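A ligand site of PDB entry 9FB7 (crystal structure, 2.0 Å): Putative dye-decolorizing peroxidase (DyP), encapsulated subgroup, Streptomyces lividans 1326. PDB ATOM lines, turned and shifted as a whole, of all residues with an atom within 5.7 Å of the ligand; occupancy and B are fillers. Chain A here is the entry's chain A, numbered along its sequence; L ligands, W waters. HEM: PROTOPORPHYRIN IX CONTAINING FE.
The backbone carbonyl oxygen (O) of His 225 sits at hydrogen-bond distance from the side-chain hydroxyl (OG1) of Thr 229. The side-chain carboxylate (OD2) of Asp 212 is in hydrogen-bond range of the side-chain hydroxyl (OG1) of Thr 154 (2.6 Å). OG of Ser 230 is in hydrogen-bond range of O of Val 226 (2.8 Å). The guanidinium group (NE) of Arg 207 lies within salt-bridge range of the side-chain carboxylate (OD1) of Asp 212 (2.9 Å). OH of Tyr 186 sits at hydrogen-bond distance from OE1 of Gln 184 (2.7 Å). NH1 of Arg 243 lies within salt-bridge range of OD1 of Asp 152 (3.7 Å). OD2 of Asp 146 sits close to OD2 of Asp 152. The side-chain carboxylate (OD1) of Asp 152 is in hydrogen-bond range of the side-chain amide nitrogen (ND2) of Asn 245, at 3.2 Å.
Water W3 lies within hydrogen-bond range of the side-chain amide nitrogen of Asn 245 and the guanidinium group of Arg 243. Water W1 bridges an oxygen (O2D) of the ligand (2.7 Å) and the guanidinium group (NH1) of Arg 207 (3.1 Å). Water W2 bridges the backbone carbonyl oxygen of Thr 229 and an oxygen (O1D) of the ligand.
The backbone NH (N) of Glu 155 lies within hydrogen-bond range of an oxygen (O2A) of the ligand (3.0 Å). A ring nitrogen (NE2) of His 225 is bound to an iron atom (FE) of the ligand, 2.1 Å away. NH1 of Arg 243 is in salt-bridge range of O1A of the ligand (3.0 Å). N of Gly 153 sits at hydrogen-bond distance from O1A of the ligand (2.6 Å). An oxygen (O1A) of the ligand is in hydrogen-bond range of the backbone NH (N) of Thr 154, at 3.2 Å.
Residues that only touch the ligand: Asp 146 (3.3 Å), Leu 148 (3.96 Å), Phe 150 (3.8 Å), Val 151 (3.3 Å), Asp 152 (3.4 Å), Gln 184 (3.5 Å), Tyr 186 (3.3 Å), Arg 207 (3.5 Å), Val 226 (3.96 Å), Thr 229 (3.4 Å), Ser 230 (3.5 Å), Asn 245 (3.8 Å), Thr 258 (3.8 Å), Phe 260 (3.4 Å), Met 273 (3.8 Å), Leu 274 (3.9 Å), Met 277 (3.7 Å) and Ile 289 (3.6 Å). Hydrophobic or aromatic side chains within 4 Å of the ligand: Leu 148, Phe 150, Tyr 186, His 225, Val 226, Phe 260, Met 273, Leu 274, Met 277 and Ile 289. The nearest printed residue that does not touch the ligand is Thr 270 (4.02 Å).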
ATOM      1  N   ASP A 146     -24.330  -1.630 -27.683  1.00  0.00           N
ATOM      2  CA  ASP A 146     -23.459  -2.101 -26.641  1.00  0.00           C
ATOM      3  C   ASP A 146     -22.111  -2.359 -27.282  1.00  0.00           C
ATOM      4  O   ASP A 146     -21.895  -2.042 -28.434  1.00  0.00           O
ATOM      5  CB  ASP A 146     -24.049  -3.293 -25.908  1.00  0.00           C
ATOM      6  CG  ASP A 146     -24.319  -4.502 -26.777  1.00  0.00           C
ATOM      7  OD1 ASP A 146     -23.665  -4.597 -27.834  1.00  0.00           O
ATOM      8  OD2 ASP A 146     -25.226  -5.258 -26.411  1.00  0.00           O
ATOM      9  N   LEU A 148     -20.732  -4.991 -28.214  1.00  0.00           N
ATOM     10  CA  LEU A 148     -20.703  -5.946 -29.315  1.00  0.00           C
ATOM     11  C   LEU A 148     -21.330  -5.353 -30.583  1.00  0.00           C
ATOM     12  O   LEU A 148     -21.426  -6.037 -31.577  1.00  0.00           O
ATOM     13  CB  LEU A 148     -21.476  -7.195 -28.909  1.00  0.00           C
ATOM     14  CG  LEU A 148     -21.035  -7.893 -27.618  1.00  0.00           C
ATOM     15  CD1 LEU A 148     -22.033  -8.986 -27.324  1.00  0.00           C
ATOM     16  CD2 LEU A 148     -19.620  -8.421 -27.756  1.00  0.00           C
ATOM     17  N   PHE A 150     -24.494  -4.248 -31.116  1.00  0.00           N
ATOM     18  CA  PHE A 150     -25.928  -4.450 -31.257  1.00  0.00           C
ATOM     19  C   PHE A 150     -26.713  -3.468 -30.398  1.00  0.00           C
ATOM     20  O   PHE A 150     -26.266  -3.107 -29.309  1.00  0.00           O
ATOM     21  CB  PHE A 150     -26.310  -5.864 -30.849  1.00  0.00           C
ATOM     22  CG  PHE A 150     -26.036  -6.886 -31.941  1.00  0.00           C
ATOM     23  CD1 PHE A 150     -24.739  -7.264 -32.222  1.00  0.00           C
ATOM     24  CD2 PHE A 150     -27.065  -7.468 -32.653  1.00  0.00           C
ATOM     25  CE1 PHE A 150     -24.498  -8.192 -33.235  1.00  0.00           C
ATOM     26  CE2 PHE A 150     -26.812  -8.386 -33.658  1.00  0.00           C
ATOM     27  CZ  PHE A 150     -25.533  -8.723 -33.962  1.00  0.00           C
ATOM     28  N   VAL A 151     -27.905  -3.080 -30.855  1.00  0.00           N
ATOM     29  CA  VAL A 151     -28.796  -2.255 -30.061  1.00  0.00           C
ATOM     30  C   VAL A 151     -29.261  -3.090 -28.868  1.00  0.00           C
ATOM     31  O   VAL A 151     -29.647  -4.247 -29.033  1.00  0.00           O
ATOM     32  CB  VAL A 151     -29.998  -1.748 -30.871  1.00  0.00           C
ATOM     33  CG1 VAL A 151     -30.885  -0.835 -30.051  1.00  0.00           C
ATOM     34  CG2 VAL A 151     -29.599  -1.076 -32.173  1.00  0.00           C
ATOM     35  N   ASP A 152     -29.230  -2.441 -27.702  1.00  0.00           N
ATOM     36  CA  ASP A 152     -29.358  -3.069 -26.390  1.00  0.00           C
ATOM     37  C   ASP A 152     -30.403  -2.287 -25.598  1.00  0.00           C
ATOM     38  O   ASP A 152     -30.182  -1.151 -25.210  1.00  0.00           O
ATOM     39  CB  ASP A 152     -27.974  -3.110 -25.722  1.00  0.00           C
ATOM     40  CG  ASP A 152     -27.849  -3.971 -24.467  1.00  0.00           C
ATOM     41  OD1 ASP A 152     -28.819  -3.941 -23.659  1.00  0.00           O
ATOM     42  OD2 ASP A 152     -26.757  -4.640 -24.295  1.00  0.00           O
ATOM     43  N   GLY A 153     -31.531  -2.928 -25.337  1.00  0.00           N
ATOM     44  CA  GLY A 153     -32.631  -2.301 -24.614  1.00  0.00           C
ATOM     45  C   GLY A 153     -33.999  -2.490 -25.294  1.00  0.00           C
ATOM     46  O   GLY A 153     -34.995  -2.226 -24.659  1.00  0.00           O
ATOM     47  N   THR A 154     -34.060  -2.973 -26.543  1.00  0.00           N
ATOM     48  CA  THR A 154     -35.193  -2.789 -27.448  1.00  0.00           C
ATOM     49  C   THR A 154     -36.449  -3.435 -26.902  1.00  0.00           C
ATOM     50  O   THR A 154     -37.527  -2.856 -26.960  1.00  0.00           O
ATOM     51  CB  THR A 154     -34.843  -3.439 -28.774  1.00  0.00           C
ATOM     52  OG1 THR A 154     -33.586  -2.895 -29.182  1.00  0.00           O
ATOM     53  CG2 THR A 154     -35.941  -3.244 -29.813  1.00  0.00           C
ATOM     54  N   GLU A 155     -36.325  -4.666 -26.405  1.00  0.00           N
ATOM     55  CA  GLU A 155     -37.464  -5.418 -25.900  1.00  0.00           C
ATOM     56  C   GLU A 155     -37.709  -5.210 -24.408  1.00  0.00           C
ATOM     57  O   GLU A 155     -38.494  -5.922 -23.823  1.00  0.00           O
ATOM     58  CB  GLU A 155     -37.308  -6.902 -26.254  1.00  0.00           C
ATOM     59  CG  GLU A 155     -37.600  -7.169 -27.744  1.00  0.00           C
ATOM     60  CD  GLU A 155     -39.038  -6.864 -28.085  1.00  0.00           C
ATOM     61  OE1 GLU A 155     -39.886  -7.483 -27.413  1.00  0.00           O
ATOM     62  OE2 GLU A 155     -39.286  -5.971 -28.885  1.00  0.00           O
ATOM     63  N   ASN A 156     -37.142  -4.189 -23.762  1.00  0.00           N
ATOM     64  CA  ASN A 156     -37.527  -3.913 -22.392  1.00  0.00           C
ATOM     65  C   ASN A 156     -39.005  -3.562 -22.313  1.00  0.00           C
ATOM     66  O   ASN A 156     -39.510  -2.870 -23.170  1.00  0.00           O
ATOM     67  CB  ASN A 156     -36.805  -2.715 -21.798  1.00  0.00           C
ATOM     68  CG  ASN A 156     -35.528  -3.110 -21.116  1.00  0.00           C
ATOM     69  OD1 ASN A 156     -35.454  -4.173 -20.477  1.00  0.00           O
ATOM     70  ND2 ASN A 156     -34.538  -2.251 -21.247  1.00  0.00           N
ATOM     71  N   GLN A 184     -24.161  -7.968 -12.881  1.00  0.00           N
ATOM     72  CA  GLN A 184     -22.997  -8.717 -13.319  1.00  0.00           C
ATOM     73  C   GLN A 184     -22.129  -7.839 -14.217  1.00  0.00           C
ATOM     74  O   GLN A 184     -22.607  -7.228 -15.172  1.00  0.00           O
ATOM     75  CB  GLN A 184     -23.379  -9.931 -14.146  1.00  0.00           C
ATOM     76  CG  GLN A 184     -24.153 -11.008 -13.384  1.00  0.00           C
ATOM     77  CD  GLN A 184     -24.412 -12.175 -14.284  1.00  0.00           C
ATOM     78  OE1 GLN A 184     -25.182 -12.021 -15.232  1.00  0.00           O
ATOM     79  NE2 GLN A 184     -23.671 -13.274 -14.055  1.00  0.00           N
ATOM     80  N   TYR A 186     -19.551  -7.839 -17.072  1.00  0.00           N
ATOM     81  CA  TYR A 186     -19.040  -8.721 -18.116  1.00  0.00           C
ATOM     82  C   TYR A 186     -17.892  -8.051 -18.860  1.00  0.00           C
ATOM     83  O   TYR A 186     -17.961  -6.863 -19.167  1.00  0.00           O
ATOM     84  CB  TYR A 186     -20.097  -9.066 -19.156  1.00  0.00           C
ATOM     85  CG  TYR A 186     -21.094 -10.112 -18.703  1.00  0.00           C
ATOM     86  CD1 TYR A 186     -20.860 -11.459 -18.871  1.00  0.00           C
ATOM     87  CD2 TYR A 186     -22.290  -9.718 -18.096  1.00  0.00           C
ATOM     88  CE1 TYR A 186     -21.792 -12.399 -18.470  1.00  0.00           C
ATOM     89  CE2 TYR A 186     -23.206 -10.643 -17.635  1.00  0.00           C
ATOM     90  CZ  TYR A 186     -22.961 -11.997 -17.838  1.00  0.00           C
ATOM     91  OH  TYR A 186     -23.916 -12.888 -17.437  1.00  0.00           O
ATOM     92  N   HIS A 188     -15.757  -8.566 -22.514  1.00  0.00           N
ATOM     93  CA  HIS A 188     -15.912  -9.229 -23.791  1.00  0.00           C
ATOM     94  C   HIS A 188     -14.549  -9.458 -24.412  1.00  0.00           C
ATOM     95  O   HIS A 188     -13.641  -8.657 -24.213  1.00  0.00           O
ATOM     96  CB  HIS A 188     -16.751  -8.384 -24.740  1.00  0.00           C
ATOM     97  CG  HIS A 188     -18.127  -8.116 -24.237  1.00  0.00           C
ATOM     98  ND1 HIS A 188     -19.061  -9.109 -24.183  1.00  0.00           N
ATOM     99  CD2 HIS A 188     -18.714  -6.989 -23.767  1.00  0.00           C
ATOM    100  CE1 HIS A 188     -20.200  -8.592 -23.728  1.00  0.00           C
ATOM    101  NE2 HIS A 188     -20.008  -7.306 -23.457  1.00  0.00           N
ATOM    102  N   ILE A 205     -26.901 -13.433 -31.294  1.00  0.00           N
ATOM    103  CA  ILE A 205     -27.784 -12.564 -30.542  1.00  0.00           C
ATOM    104  C   ILE A 205     -29.234 -12.971 -30.766  1.00  0.00           C
ATOM    105  O   ILE A 205     -30.003 -13.060 -29.816  1.00  0.00           O
ATOM    106  CB  ILE A 205     -27.511 -11.095 -30.925  1.00  0.00           C
ATOM    107  CG1 ILE A 205     -26.090 -10.705 -30.620  1.00  0.00           C
ATOM    108  CG2 ILE A 205     -28.501 -10.129 -30.280  1.00  0.00           C
ATOM    109  CD1 ILE A 205     -25.753 -10.636 -29.147  1.00  0.00           C
ATOM    110  N   ARG A 207     -30.995 -11.247 -33.368  1.00  0.00           N
ATOM    111  CA  ARG A 207     -31.584 -10.108 -34.054  1.00  0.00           C
ATOM    112  C   ARG A 207     -30.612  -9.626 -35.115  1.00  0.00           C
ATOM    113  O   ARG A 207     -29.444  -9.961 -35.075  1.00  0.00           O
ATOM    114  CB  ARG A 207     -31.788  -8.956 -33.065  1.00  0.00           C
ATOM    115  CG  ARG A 207     -32.556  -9.330 -31.813  1.00  0.00           C
ATOM    116  CD  ARG A 207     -32.858  -8.163 -30.910  1.00  0.00           C
ATOM    117  NE  ARG A 207     -33.828  -7.191 -31.459  1.00  0.00           N
ATOM    118  CZ  ARG A 207     -35.151  -7.233 -31.328  1.00  0.00           C
ATOM    119  NH1 ARG A 207     -35.789  -8.180 -30.656  1.00  0.00           N
ATOM    120  NH2 ARG A 207     -35.859  -6.269 -31.867  1.00  0.00           N
ATOM    121  N   ASP A 212     -31.830  -4.023 -36.172  1.00  0.00           N
ATOM    122  CA  ASP A 212     -32.390  -4.456 -34.890  1.00  0.00           C
ATOM    123  C   ASP A 212     -33.768  -5.098 -35.038  1.00  0.00           C
ATOM    124  O   ASP A 212     -34.573  -5.034 -34.118  1.00  0.00           O
ATOM    125  CB  ASP A 212     -32.562  -3.313 -33.900  1.00  0.00           C
ATOM    126  CG  ASP A 212     -32.742  -3.664 -32.438  1.00  0.00           C
ATOM    127  OD1 ASP A 212     -32.253  -4.785 -31.994  1.00  0.00           O
ATOM    128  OD2 ASP A 212     -33.286  -2.723 -31.765  1.00  0.00           O
ATOM    129  N   GLU A 214     -35.904  -8.540 -35.089  1.00  0.00           N
ATOM    130  CA  GLU A 214     -35.748  -9.894 -34.569  1.00  0.00           C
ATOM    131  C   GLU A 214     -35.636 -10.893 -35.718  1.00  0.00           C
ATOM    132  O   GLU A 214     -36.277 -10.743 -36.723  1.00  0.00           O
ATOM    133  CB  GLU A 214     -37.003 -10.151 -33.743  1.00  0.00           C
ATOM    134  CG  GLU A 214     -36.912 -11.402 -32.884  1.00  0.00           C
ATOM    135  CD  GLU A 214     -37.928 -11.418 -31.764  1.00  0.00           C
ATOM    136  OE1 GLU A 214     -38.542 -10.396 -31.367  1.00  0.00           O
ATOM    137  OE2 GLU A 214     -38.046 -12.513 -31.261  1.00  0.00           O
ATOM    138  N   HIS A 225     -29.118 -15.650 -27.865  1.00  0.00           N
ATOM    139  CA  HIS A 225     -29.308 -14.982 -26.594  1.00  0.00           C
ATOM    140  C   HIS A 225     -30.781 -14.651 -26.392  1.00  0.00           C
ATOM    141  O   HIS A 225     -31.307 -14.828 -25.287  1.00  0.00           O
ATOM    142  CB  HIS A 225     -28.409 -13.749 -26.515  1.00  0.00           C
ATOM    143  CG  HIS A 225     -28.595 -12.928 -25.286  1.00  0.00           C
ATOM    144  ND1 HIS A 225     -28.342 -13.405 -24.039  1.00  0.00           N
ATOM    145  CD2 HIS A 225     -29.002 -11.674 -25.118  1.00  0.00           C
ATOM    146  CE1 HIS A 225     -28.577 -12.456 -23.151  1.00  0.00           C
ATOM    147  NE2 HIS A 225     -28.983 -11.388 -23.789  1.00  0.00           N
ATOM    148  N   VAL A 226     -31.444 -14.214 -27.474  1.00  0.00           N
ATOM    149  CA  VAL A 226     -32.839 -13.821 -27.393  1.00  0.00           C
ATOM    150  C   VAL A 226     -33.729 -15.044 -27.213  1.00  0.00           C
ATOM    151  O   VAL A 226     -34.773 -14.971 -26.589  1.00  0.00           O
ATOM    152  CB  VAL A 226     -33.230 -13.006 -28.638  1.00  0.00           C
ATOM    153  CG1 VAL A 226     -34.727 -13.049 -28.906  1.00  0.00           C
ATOM    154  CG2 VAL A 226     -32.758 -11.555 -28.496  1.00  0.00           C
ATOM    155  N   THR A 229     -33.347 -16.136 -23.402  1.00  0.00           N
ATOM    156  CA  THR A 229     -33.801 -15.222 -22.371  1.00  0.00           C
ATOM    157  C   THR A 229     -35.286 -14.878 -22.582  1.00  0.00           C
ATOM    158  O   THR A 229     -35.785 -14.043 -21.836  1.00  0.00           O
ATOM    159  CB  THR A 229     -32.935 -13.967 -22.334  1.00  0.00           C
ATOM    160  OG1 THR A 229     -32.998 -13.323 -23.622  1.00  0.00           O
ATOM    161  CG2 THR A 229     -31.514 -14.259 -21.904  1.00  0.00           C
ATOM    162  N   SER A 230     -35.960 -15.514 -23.554  1.00  0.00           N
ATOM    163  CA  SER A 230     -37.408 -15.458 -23.672  1.00  0.00           C
ATOM    164  C   SER A 230     -38.005 -16.604 -22.881  1.00  0.00           C
ATOM    165  O   SER A 230     -37.694 -17.754 -23.118  1.00  0.00           O
ATOM    166  CB  SER A 230     -37.855 -15.532 -25.093  1.00  0.00           C
ATOM    167  OG  SER A 230     -37.448 -14.393 -25.820  1.00  0.00           O
ATOM    168  N   ILE A 241     -38.056  -8.848 -17.499  1.00  0.00           N
ATOM    169  CA  ILE A 241     -37.274  -8.005 -16.594  1.00  0.00           C
ATOM    170  C   ILE A 241     -36.997  -6.645 -17.236  1.00  0.00           C
ATOM    171  O   ILE A 241     -37.202  -6.433 -18.423  1.00  0.00           O
ATOM    172  CB  ILE A 241     -35.961  -8.698 -16.194  1.00  0.00           C
ATOM    173  CG1 ILE A 241     -35.010  -8.851 -17.350  1.00  0.00           C
ATOM    174  CG2 ILE A 241     -36.242 -10.040 -15.528  1.00  0.00           C
ATOM    175  CD1 ILE A 241     -33.654  -9.385 -16.919  1.00  0.00           C
ATOM    176  N   ARG A 243     -33.915  -4.087 -17.978  1.00  0.00           N
ATOM    177  CA  ARG A 243     -32.476  -4.030 -18.026  1.00  0.00           C
ATOM    178  C   ARG A 243     -32.011  -2.614 -18.322  1.00  0.00           C
ATOM    179  O   ARG A 243     -32.711  -1.871 -18.974  1.00  0.00           O
ATOM    180  CB  ARG A 243     -31.961  -4.914 -19.166  1.00  0.00           C
ATOM    181  CG  ARG A 243     -32.214  -6.391 -18.935  1.00  0.00           C
ATOM    182  CD  ARG A 243     -31.944  -7.189 -20.197  1.00  0.00           C
ATOM    183  NE  ARG A 243     -33.003  -6.918 -21.158  1.00  0.00           N
ATOM    184  CZ  ARG A 243     -32.799  -6.417 -22.366  1.00  0.00           C
ATOM    185  NH1 ARG A 243     -31.566  -6.259 -22.838  1.00  0.00           N
ATOM    186  NH2 ARG A 243     -33.850  -6.124 -23.110  1.00  0.00           N
ATOM    187  N   ASN A 245     -28.340  -2.126 -19.282  1.00  0.00           N
ATOM    188  CA  ASN A 245     -26.937  -2.414 -19.544  1.00  0.00           C
ATOM    189  C   ASN A 245     -26.199  -1.151 -20.001  1.00  0.00           C
ATOM    190  O   ASN A 245     -26.720  -0.371 -20.827  1.00  0.00           O
ATOM    191  CB  ASN A 245     -26.786  -3.478 -20.636  1.00  0.00           C
ATOM    192  CG  ASN A 245     -27.508  -4.746 -20.236  1.00  0.00           C
ATOM    193  OD1 ASN A 245     -27.913  -4.896 -19.069  1.00  0.00           O
ATOM    194  ND2 ASN A 245     -27.673  -5.666 -21.175  1.00  0.00           N
ATOM    195  N   THR A 258     -19.678  -4.891 -20.721  1.00  0.00           N
ATOM    196  CA  THR A 258     -21.077  -4.556 -20.550  1.00  0.00           C
ATOM    197  C   THR A 258     -21.361  -4.739 -19.067  1.00  0.00           C
ATOM    198  O   THR A 258     -21.076  -5.801 -18.529  1.00  0.00           O
ATOM    199  CB  THR A 258     -21.950  -5.451 -21.454  1.00  0.00           C
ATOM    200  OG1 THR A 258     -21.749  -5.096 -22.839  1.00  0.00           O
ATOM    201  CG2 THR A 258     -23.418  -5.377 -21.044  1.00  0.00           C
ATOM    202  N   PHE A 260     -24.160  -5.404 -16.720  1.00  0.00           N
ATOM    203  CA  PHE A 260     -25.528  -5.867 -16.733  1.00  0.00           C
ATOM    204  C   PHE A 260     -26.213  -5.501 -15.418  1.00  0.00           C
ATOM    205  O   PHE A 260     -25.685  -5.789 -14.349  1.00  0.00           O
ATOM    206  CB  PHE A 260     -25.546  -7.379 -16.894  1.00  0.00           C
ATOM    207  CG  PHE A 260     -26.927  -7.921 -16.669  1.00  0.00           C
ATOM    208  CD1 PHE A 260     -27.879  -7.875 -17.689  1.00  0.00           C
ATOM    209  CD2 PHE A 260     -27.295  -8.465 -15.460  1.00  0.00           C
ATOM    210  CE1 PHE A 260     -29.162  -8.364 -17.477  1.00  0.00           C
ATOM    211  CE2 PHE A 260     -28.571  -8.953 -15.261  1.00  0.00           C
ATOM    212  CZ  PHE A 260     -29.499  -8.908 -16.267  1.00  0.00           C
ATOM    213  N   THR A 270     -35.261 -13.499 -12.982  1.00  0.00           N
ATOM    214  CA  THR A 270     -33.898 -13.201 -13.418  1.00  0.00           C
ATOM    215  C   THR A 270     -33.066 -14.468 -13.332  1.00  0.00           C
ATOM    216  O   THR A 270     -32.264 -14.726 -14.214  1.00  0.00           O
ATOM    217  CB  THR A 270     -33.307 -12.086 -12.564  1.00  0.00           C
ATOM    218  OG1 THR A 270     -34.081 -10.894 -12.567  1.00  0.00           O
ATOM    219  CG2 THR A 270     -32.003 -11.576 -13.144  1.00  0.00           C
ATOM    220  N   MET A 273     -33.582 -17.040 -16.162  1.00  0.00           N
ATOM    221  CA  MET A 273     -32.911 -16.640 -17.385  1.00  0.00           C
ATOM    222  C   MET A 273     -31.426 -16.968 -17.246  1.00  0.00           C
ATOM    223  O   MET A 273     -30.795 -17.465 -18.181  1.00  0.00           O
ATOM    224  CB  MET A 273     -33.108 -15.139 -17.622  1.00  0.00           C
ATOM    225  CG  MET A 273     -34.515 -14.722 -17.985  1.00  0.00           C
ATOM    226  SD  MET A 273     -34.697 -12.926 -18.017  1.00  0.00           S
ATOM    227  CE  MET A 273     -36.434 -12.727 -18.479  1.00  0.00           C
ATOM    228  N   LEU A 274     -30.865 -16.702 -16.061  1.00  0.00           N
ATOM    229  CA  LEU A 274     -29.464 -16.958 -15.841  1.00  0.00           C
ATOM    230  C   LEU A 274     -29.129 -18.448 -15.965  1.00  0.00           C
ATOM    231  O   LEU A 274     -28.075 -18.798 -16.519  1.00  0.00           O
ATOM    232  CB  LEU A 274     -29.080 -16.419 -14.471  1.00  0.00           C
ATOM    233  CG  LEU A 274     -28.715 -14.943 -14.411  1.00  0.00           C
ATOM    234  CD1 LEU A 274     -28.547 -14.435 -12.962  1.00  0.00           C
ATOM    235  CD2 LEU A 274     -27.386 -14.771 -15.170  1.00  0.00           C
ATOM    236  N   MET A 277     -29.036 -19.479 -19.487  1.00  0.00           N
ATOM    237  CA  MET A 277     -27.883 -18.992 -20.203  1.00  0.00           C
ATOM    238  C   MET A 277     -26.659 -19.833 -19.842  1.00  0.00           C
ATOM    239  O   MET A 277     -25.890 -20.213 -20.713  1.00  0.00           O
ATOM    240  CB  MET A 277     -27.594 -17.517 -19.893  1.00  0.00           C
ATOM    241  CG  MET A 277     -28.564 -16.510 -20.511  1.00  0.00           C
ATOM    242  SD  MET A 277     -28.242 -14.886 -19.803  1.00  0.00           S
ATOM    243  CE  MET A 277     -26.588 -14.568 -20.423  1.00  0.00           C
ATOM    244  N   ILE A 289     -23.689 -16.084 -26.349  1.00  0.00           N
ATOM    245  CA  ILE A 289     -23.097 -14.806 -26.024  1.00  0.00           C
ATOM    246  C   ILE A 289     -21.995 -14.993 -24.974  1.00  0.00           C
ATOM    247  O   ILE A 289     -21.091 -14.151 -24.896  1.00  0.00           O
ATOM    248  CB  ILE A 289     -24.179 -13.807 -25.559  1.00  0.00           C
ATOM    249  CG1 ILE A 289     -23.765 -12.373 -25.849  1.00  0.00           C
ATOM    250  CG2 ILE A 289     -24.505 -13.972 -24.073  1.00  0.00           C
ATOM    251  CD1 ILE A 289     -24.806 -11.315 -25.486  1.00  0.00           C
ATOM    252  N   LEU A 290     -22.071 -16.072 -24.169  1.00  0.00           N
ATOM    253  CA  LEU A 290     -21.092 -16.340 -23.122  1.00  0.00           C
ATOM    254  C   LEU A 290     -19.784 -16.863 -23.719  1.00  0.00           C
ATOM    255  O   LEU A 290     -18.759 -16.859 -23.061  1.00  0.00           O
ATOM    256  CB  LEU A 290     -21.639 -17.334 -22.094  1.00  0.00           C
ATOM    257  CG  LEU A 290     -22.874 -16.852 -21.354  1.00  0.00           C
ATOM    258  CD1 LEU A 290     -23.342 -17.956 -20.430  1.00  0.00           C
ATOM    259  CD2 LEU A 290     -22.560 -15.584 -20.577  1.00  0.00           C
ATOM    260  N   SER A 293     -18.206 -13.451 -23.658  1.00  0.00           N
ATOM    261  CA  SER A 293     -18.483 -12.593 -22.525  1.00  0.00           C
ATOM    262  C   SER A 293     -18.160 -13.381 -21.259  1.00  0.00           C
ATOM    263  O   SER A 293     -18.692 -14.475 -21.118  1.00  0.00           O
ATOM    264  CB  SER A 293     -19.920 -12.136 -22.512  1.00  0.00           C
ATOM    265  OG  SER A 293     -20.340 -11.788 -23.815  1.00  0.00           O
HETATM  266  CHA HEM L   1     -31.932  -8.951 -25.001  1.00  0.00           C
HETATM  267  CHB HEM L   1     -27.195  -7.900 -25.011  1.00  0.00           C
HETATM  268  CHC HEM L   1     -26.666 -10.154 -20.684  1.00  0.00           C
HETATM  269  CHD HEM L   1     -31.498 -10.713 -20.578  1.00  0.00           C
HETATM  270  C1A HEM L   1     -30.653  -8.499 -25.381  1.00  0.00           C
HETATM  271  C2A HEM L   1     -30.355  -7.921 -26.651  1.00  0.00           C
HETATM  272  C3A HEM L   1     -29.024  -7.569 -26.636  1.00  0.00           C
HETATM  273  C4A HEM L   1     -28.486  -7.980 -25.402  1.00  0.00           C
HETATM  274  CMA HEM L   1     -28.316  -6.945 -27.769  1.00  0.00           C
HETATM  275  CAA HEM L   1     -31.378  -7.729 -27.754  1.00  0.00           C
HETATM  276  CBA HEM L   1     -32.043  -6.348 -27.712  1.00  0.00           C
HETATM  277  CGA HEM L   1     -32.842  -6.108 -26.488  1.00  0.00           C
HETATM  278  O1A HEM L   1     -32.268  -5.404 -25.639  1.00  0.00           O
HETATM  279  O2A HEM L   1     -34.033  -6.564 -26.425  1.00  0.00           O
HETATM  280  C1B HEM L   1     -26.668  -8.457 -23.837  1.00  0.00           C
HETATM  281  C2B HEM L   1     -25.307  -8.350 -23.526  1.00  0.00           C
HETATM  282  C3B HEM L   1     -25.109  -8.936 -22.303  1.00  0.00           C
HETATM  283  C4B HEM L   1     -26.431  -9.454 -21.864  1.00  0.00           C
HETATM  284  CMB HEM L   1     -24.269  -7.624 -24.359  1.00  0.00           C
HETATM  285  CAB HEM L   1     -23.736  -9.097 -21.766  1.00  0.00           C
HETATM  286  CBB HEM L   1     -23.301 -10.237 -21.225  1.00  0.00           C
HETATM  287  C1C HEM L   1     -27.908 -10.521 -20.235  1.00  0.00           C
HETATM  288  C2C HEM L   1     -28.259 -11.223 -19.063  1.00  0.00           C
HETATM  289  C3C HEM L   1     -29.651 -11.397 -19.047  1.00  0.00           C
HETATM  290  C4C HEM L   1     -30.141 -10.769 -20.226  1.00  0.00           C
HETATM  291  CMC HEM L   1     -27.294 -11.682 -18.016  1.00  0.00           C
HETATM  292  CAC HEM L   1     -30.628 -11.978 -18.127  1.00  0.00           C
HETATM  293  CBC HEM L   1     -30.365 -12.479 -16.958  1.00  0.00           C
HETATM  294  C1D HEM L   1     -32.017 -10.264 -21.773  1.00  0.00           C
HETATM  295  C2D HEM L   1     -33.424 -10.305 -22.055  1.00  0.00           C
HETATM  296  C3D HEM L   1     -33.585  -9.856 -23.310  1.00  0.00           C
HETATM  297  C4D HEM L   1     -32.194  -9.527 -23.751  1.00  0.00           C
HETATM  298  CMD HEM L   1     -34.505 -10.749 -21.116  1.00  0.00           C
HETATM  299  CAD HEM L   1     -34.879  -9.632 -24.115  1.00  0.00           C
HETATM  300  CBD HEM L   1     -35.506 -10.945 -24.755  1.00  0.00           C
HETATM  301  CGD HEM L   1     -36.798 -10.749 -25.594  1.00  0.00           C
HETATM  302  O1D HEM L   1     -38.023 -10.964 -25.285  1.00  0.00           O
HETATM  303  O2D HEM L   1     -36.596 -10.303 -26.743  1.00  0.00           O
HETATM  304  NA  HEM L   1     -29.453  -8.559 -24.631  1.00  0.00           N
HETATM  305  NB  HEM L   1     -27.290  -9.109 -22.845  1.00  0.00           N
HETATM  306  NC  HEM L   1     -29.063 -10.265 -20.910  1.00  0.00           N
HETATM  307  ND  HEM L   1     -31.287  -9.801 -22.778  1.00  0.00           N
HETATM  308 FE   HEM L   1     -29.358  -9.552 -22.867  1.00  0.00          FE
HETATM  309  O   HOH W   1     -34.608  -8.903 -27.908  1.00  0.00           O
HETATM  310  O   HOH W   2     -37.300 -11.680 -22.209  1.00  0.00           O
HETATM  311  O   HOH W   3     -29.228  -7.854 -21.984  1.00  0.00           O
